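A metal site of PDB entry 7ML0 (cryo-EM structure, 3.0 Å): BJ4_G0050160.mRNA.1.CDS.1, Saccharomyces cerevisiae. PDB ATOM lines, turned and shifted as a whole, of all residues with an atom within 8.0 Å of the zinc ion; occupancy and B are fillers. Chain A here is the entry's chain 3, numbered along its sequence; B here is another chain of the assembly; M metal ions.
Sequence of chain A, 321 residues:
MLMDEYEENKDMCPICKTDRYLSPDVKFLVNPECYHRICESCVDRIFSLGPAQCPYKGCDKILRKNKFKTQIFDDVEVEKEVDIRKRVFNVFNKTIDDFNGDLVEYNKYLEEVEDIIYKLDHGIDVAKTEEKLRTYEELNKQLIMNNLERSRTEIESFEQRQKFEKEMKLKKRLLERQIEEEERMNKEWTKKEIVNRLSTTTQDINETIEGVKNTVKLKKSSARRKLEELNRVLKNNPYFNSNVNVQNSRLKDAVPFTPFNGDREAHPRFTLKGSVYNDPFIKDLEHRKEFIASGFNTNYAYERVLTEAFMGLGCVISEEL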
ATOM      1  N   MET A  12       2.494 -14.689   6.715  1.00  0.00           N
ATOM      2  CA  MET A  12       2.384 -14.676   8.164  1.00  0.00           C
ATOM      3  C   MET A  12       3.761 -14.447   8.764  1.00  0.00           C
ATOM      4  O   MET A  12       4.783 -14.852   8.192  1.00  0.00           O
ATOM      5  CB  MET A  12       1.788 -15.989   8.699  1.00  0.00           C
ATOM      6  CG  MET A  12       2.651 -17.223   8.485  1.00  0.00           C
ATOM      7  SD  MET A  12       1.872 -18.726   9.093  1.00  0.00           S
ATOM      8  CE  MET A  12       0.484 -18.879   7.977  1.00  0.00           C
ATOM      9  N   CYS A  13       3.786 -13.780   9.916  1.00  0.00           N
ATOM     10  CA  CYS A  13       5.048 -13.449  10.560  1.00  0.00           C
ATOM     11  C   CYS A  13       5.780 -14.724  10.959  1.00  0.00           C
ATOM     12  O   CYS A  13       5.201 -15.559  11.668  1.00  0.00           O
ATOM     13  CB  CYS A  13       4.807 -12.574  11.785  1.00  0.00           C
ATOM     14  SG  CYS A  13       6.295 -12.172  12.707  1.00  0.00           S
ATOM     15  N   PRO A  14       7.027 -14.908  10.535  1.00  0.00           N
ATOM     16  CA  PRO A  14       7.783 -16.087  10.999  1.00  0.00           C
ATOM     17  C   PRO A  14       7.897 -16.188  12.517  1.00  0.00           C
ATOM     18  O   PRO A  14       8.339 -17.225  13.023  1.00  0.00           O
ATOM     19  CB  PRO A  14       9.146 -15.906  10.321  1.00  0.00           C
ATOM     20  CG  PRO A  14       8.823 -15.172   9.065  1.00  0.00           C
ATOM     21  CD  PRO A  14       7.697 -14.232   9.418  1.00  0.00           C
ATOM     22  N   ILE A  15       7.530 -15.147  13.251  1.00  0.00           N
ATOM     23  CA  ILE A  15       7.629 -15.172  14.707  1.00  0.00           C
ATOM     24  C   ILE A  15       6.310 -15.654  15.305  1.00  0.00           C
ATOM     25  O   ILE A  15       6.251 -16.688  15.966  1.00  0.00           O
ATOM     26  CB  ILE A  15       8.020 -13.797  15.268  1.00  0.00           C
ATOM     27  CG1 ILE A  15       9.123 -13.166  14.429  1.00  0.00           C
ATOM     28  CG2 ILE A  15       8.455 -13.921  16.720  1.00  0.00           C
ATOM     29  CD1 ILE A  15      10.314 -14.063  14.213  1.00  0.00           C
ATOM     30  N   CYS A  16       5.240 -14.887  15.079  1.00  0.00           N
ATOM     31  CA  CYS A  16       3.947 -15.206  15.656  1.00  0.00           C
ATOM     32  C   CYS A  16       2.979 -15.842  14.671  1.00  0.00           C
ATOM     33  O   CYS A  16       1.885 -16.259  15.081  1.00  0.00           O
ATOM     34  CB  CYS A  16       3.309 -13.956  16.253  1.00  0.00           C
ATOM     35  SG  CYS A  16       3.365 -12.519  15.184  1.00  0.00           S
ATOM     36  N   LYS A  17       3.344 -15.940  13.389  1.00  0.00           N
ATOM     37  CA  LYS A  17       2.529 -16.602  12.365  1.00  0.00           C
ATOM     38  C   LYS A  17       1.122 -16.020  12.312  1.00  0.00           C
ATOM     39  O   LYS A  17       0.132 -16.742  12.153  1.00  0.00           O
ATOM     40  CB  LYS A  17       2.492 -18.110  12.593  1.00  0.00           C
ATOM     41  CG  LYS A  17       3.851 -18.783  12.442  1.00  0.00           C
ATOM     42  CD  LYS A  17       4.339 -19.324  13.773  1.00  0.00           C
ATOM     43  CE  LYS A  17       5.773 -19.850  13.677  1.00  0.00           C
ATOM     44  NZ  LYS A  17       6.240 -20.398  14.986  1.00  0.00           N
ATOM     45  N   THR A  18       1.026 -14.692  12.445  1.00  0.00           N
ATOM     46  CA  THR A  18      -0.251 -14.004  12.240  1.00  0.00           C
ATOM     47  C   THR A  18      -0.449 -13.852  10.741  1.00  0.00           C
ATOM     48  O   THR A  18       0.207 -13.046  10.064  1.00  0.00           O
ATOM     49  CB  THR A  18      -0.275 -12.667  12.973  1.00  0.00           C
ATOM     50  OG1 THR A  18      -1.398 -11.904  12.523  1.00  0.00           O
ATOM     51  CG2 THR A  18       1.006 -11.888  12.757  1.00  0.00           C
ATOM     52  N   VAL A  26      -1.251  -6.564   8.474  1.00  0.00           N
ATOM     53  CA  VAL A  26       0.131  -6.889   8.775  1.00  0.00           C
ATOM     54  C   VAL A  26       1.038  -6.181   7.787  1.00  0.00           C
ATOM     55  O   VAL A  26       0.769  -6.141   6.574  1.00  0.00           O
ATOM     56  CB  VAL A  26       0.355  -8.415   8.763  1.00  0.00           C
ATOM     57  CG1 VAL A  26       0.118  -8.997   7.370  1.00  0.00           C
ATOM     58  CG2 VAL A  26       1.751  -8.745   9.255  1.00  0.00           C
ATOM     59  N   PHE A  28       5.052  -6.081   6.763  1.00  0.00           N
ATOM     60  CA  PHE A  28       6.295  -6.782   6.988  1.00  0.00           C
ATOM     61  C   PHE A  28       7.466  -5.838   6.779  1.00  0.00           C
ATOM     62  O   PHE A  28       7.469  -5.001   5.883  1.00  0.00           O
ATOM     63  CB  PHE A  28       6.411  -7.986   6.067  1.00  0.00           C
ATOM     64  CG  PHE A  28       5.686  -9.191   6.572  1.00  0.00           C
ATOM     65  CD1 PHE A  28       6.362 -10.170   7.284  1.00  0.00           C
ATOM     66  CD2 PHE A  28       4.330  -9.338   6.356  1.00  0.00           C
ATOM     67  CE1 PHE A  28       5.696 -11.278   7.758  1.00  0.00           C
ATOM     68  CE2 PHE A  28       3.656 -10.446   6.825  1.00  0.00           C
ATOM     69  CZ  PHE A  28       4.335 -11.417   7.532  1.00  0.00           C
ATOM     70  N   ARG A  37      11.918 -11.732   7.494  1.00  0.00           N
ATOM     71  CA  ARG A  37      10.487 -11.525   7.424  1.00  0.00           C
ATOM     72  C   ARG A  37       9.886 -11.512   8.818  1.00  0.00           C
ATOM     73  O   ARG A  37      10.177 -12.396   9.637  1.00  0.00           O
ATOM     74  CB  ARG A  37       9.836 -12.613   6.565  1.00  0.00           C
ATOM     75  CG  ARG A  37      10.379 -12.668   5.156  1.00  0.00           C
ATOM     76  CD  ARG A  37       9.318 -13.136   4.172  1.00  0.00           C
ATOM     77  NE  ARG A  37       8.274 -12.137   3.954  1.00  0.00           N
ATOM     78  CZ  ARG A  37       7.115 -12.109   4.600  1.00  0.00           C
ATOM     79  NH1 ARG A  37       6.840 -13.034   5.512  1.00  0.00           N
ATOM     80  NH2 ARG A  37       6.225 -11.170   4.327  1.00  0.00           N
ATOM     81  N   ILE A  38       9.076 -10.495   9.105  1.00  0.00           N
ATOM     82  CA  ILE A  38       8.514 -10.327  10.434  1.00  0.00           C
ATOM     83  C   ILE A  38       7.423  -9.264  10.366  1.00  0.00           C
ATOM     84  O   ILE A  38       7.479  -8.355   9.531  1.00  0.00           O
ATOM     85  CB  ILE A  38       9.604  -9.952  11.459  1.00  0.00           C
ATOM     86  CG1 ILE A  38       9.066  -9.985  12.888  1.00  0.00           C
ATOM     87  CG2 ILE A  38      10.172  -8.575  11.159  1.00  0.00           C
ATOM     88  CD1 ILE A  38      10.153  -9.791  13.919  1.00  0.00           C
ATOM     89  N   CYS A  39       6.418  -9.396  11.222  1.00  0.00           N
ATOM     90  CA  CYS A  39       5.407  -8.353  11.355  1.00  0.00           C
ATOM     91  C   CYS A  39       5.917  -7.220  12.230  1.00  0.00           C
ATOM     92  O   CYS A  39       6.790  -7.386  13.093  1.00  0.00           O
ATOM     93  CB  CYS A  39       4.122  -8.937  11.946  1.00  0.00           C
ATOM     94  SG  CYS A  39       4.219  -9.254  13.711  1.00  0.00           S
ATOM     95  N   GLU A  40       5.342  -6.029  12.007  1.00  0.00           N
ATOM     96  CA  GLU A  40       5.733  -4.858  12.787  1.00  0.00           C
ATOM     97  C   GLU A  40       5.414  -5.047  14.258  1.00  0.00           C
ATOM     98  O   GLU A  40       6.106  -4.507  15.129  1.00  0.00           O
ATOM     99  CB  GLU A  40       5.041  -3.613  12.247  1.00  0.00           C
ATOM    100  CG  GLU A  40       5.603  -3.124  10.942  1.00  0.00           C
ATOM    101  CD  GLU A  40       4.817  -1.967  10.373  1.00  0.00           C
ATOM    102  OE1 GLU A  40       3.584  -1.918  10.614  1.00  0.00           O
ATOM    103  OE2 GLU A  40       5.413  -1.106   9.712  1.00  0.00           O
ATOM    104  N   SER A  41       4.351  -5.807  14.556  1.00  0.00           N
ATOM    105  CA  SER A  41       3.966  -6.039  15.947  1.00  0.00           C
ATOM    106  C   SER A  41       5.153  -6.533  16.767  1.00  0.00           C
ATOM    107  O   SER A  41       5.439  -6.019  17.852  1.00  0.00           O
ATOM    108  CB  SER A  41       2.813  -7.044  16.014  1.00  0.00           C
ATOM    109  OG  SER A  41       3.252  -8.273  16.565  1.00  0.00           O
ATOM    110  N   CYS A  42       5.859  -7.545  16.245  1.00  0.00           N
ATOM    111  CA  CYS A  42       7.097  -7.968  16.875  1.00  0.00           C
ATOM    112  C   CYS A  42       8.150  -6.869  16.809  1.00  0.00           C
ATOM    113  O   CYS A  42       8.837  -6.586  17.796  1.00  0.00           O
ATOM    114  CB  CYS A  42       7.599  -9.251  16.216  1.00  0.00           C
ATOM    115  SG  CYS A  42       6.488 -10.667  16.355  1.00  0.00           S
ATOM    116  N   VAL A  43       8.275  -6.216  15.651  1.00  0.00           N
ATOM    117  CA  VAL A  43       9.321  -5.226  15.394  1.00  0.00           C
ATOM    118  C   VAL A  43       9.369  -4.209  16.509  1.00  0.00           C
ATOM    119  O   VAL A  43      10.422  -3.988  17.125  1.00  0.00           O
ATOM    120  CB  VAL A  43       9.098  -4.520  14.050  1.00  0.00           C
ATOM    121  CG1 VAL A  43       9.960  -3.266  13.975  1.00  0.00           C
ATOM    122  CG2 VAL A  43       9.386  -5.453  12.891  1.00  0.00           C
ATOM    123  N   ILE A  46      10.001  -5.944  19.876  1.00  0.00           N
ATOM    124  CA  ILE A  46      11.387  -6.394  19.949  1.00  0.00           C
ATOM    125  C   ILE A  46      12.331  -5.240  20.236  1.00  0.00           C
ATOM    126  O   ILE A  46      13.218  -5.346  21.085  1.00  0.00           O
ATOM    127  CB  ILE A  46      11.758  -7.136  18.650  1.00  0.00           C
ATOM    128  CG1 ILE A  46      11.279  -8.585  18.731  1.00  0.00           C
ATOM    129  CG2 ILE A  46      13.271  -7.084  18.418  1.00  0.00           C
ATOM    130  CD1 ILE A  46      11.947  -9.385  19.828  1.00  0.00           C
ATOM    131  N   PRO A  55      14.773 -11.480  16.661  1.00  0.00           N
ATOM    132  CA  PRO A  55      13.923 -12.545  17.185  1.00  0.00           C
ATOM    133  C   PRO A  55      13.816 -13.750  16.266  1.00  0.00           C
ATOM    134  O   PRO A  55      12.728 -14.255  15.974  1.00  0.00           O
ATOM    135  CB  PRO A  55      12.562 -11.858  17.336  1.00  0.00           C
ATOM    136  CG  PRO A  55      12.575 -10.828  16.266  1.00  0.00           C
ATOM    137  CD  PRO A  55      13.980 -10.299  16.258  1.00  0.00           C
ATOM    138  N   LYS B 110      -2.911 -12.051  21.679  1.00  0.00           N
ATOM    139  CA  LYS B 110      -2.316 -10.828  21.176  1.00  0.00           C
ATOM    140  C   LYS B 110      -2.100  -9.818  22.305  1.00  0.00           C
ATOM    141  O   LYS B 110      -1.072  -9.136  22.345  1.00  0.00           O
ATOM    142  CB  LYS B 110      -3.196 -10.228  20.084  1.00  0.00           C
ATOM    143  CG  LYS B 110      -2.397  -9.578  18.971  1.00  0.00           C
ATOM    144  CD  LYS B 110      -1.329 -10.539  18.480  1.00  0.00           C
ATOM    145  CE  LYS B 110      -0.188  -9.806  17.800  1.00  0.00           C
ATOM    146  NZ  LYS B 110       0.939 -10.723  17.500  1.00  0.00           N
ATOM    147  N   LEU B 113       0.916 -11.162  24.628  1.00  0.00           N
ATOM    148  CA  LEU B 113       2.316 -10.979  24.237  1.00  0.00           C
ATOM    149  C   LEU B 113       3.016  -9.985  25.165  1.00  0.00           C
ATOM    150  O   LEU B 113       4.238 -10.037  25.332  1.00  0.00           O
ATOM    151  CB  LEU B 113       2.397 -10.516  22.785  1.00  0.00           C
ATOM    152  CG  LEU B 113       3.812 -10.437  22.185  1.00  0.00           C
ATOM    153  CD1 LEU B 113       4.274 -11.803  21.720  1.00  0.00           C
ATOM    154  CD2 LEU B 113       3.890  -9.422  21.067  1.00  0.00           C
HETATM  155 ZN    ZN M   1       5.167 -11.219  14.507  1.00  0.00          ZN
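The side-chain sulfur (SG) of Cys 39 lies close to the side-chain hydroxyl (OG) of Ser 41, at 3.2 Å.
The side-chain sulfur (SG) of Cys 13 lies close to the backbone NH (N) of Ile 15, at 3.3 Å.
Ile 15 touches the zinc ion.
Within 4 Å of the zinc ion: Cys 13, Ile 15, Cys 16, Cys 39 and Cys 42.
The nearest printed residue that does not touch the zinc ion is Ser 41 (4.1 Å).
The zinc ion is bound by SG of Cys 39 (2.3 Å), SG of Cys 16 (2.3 Å), SG of Cys 13 (2.3 Å) and SG of Cys 42 (2.3 Å).
The zinc ion has four donor atoms within binding distance.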
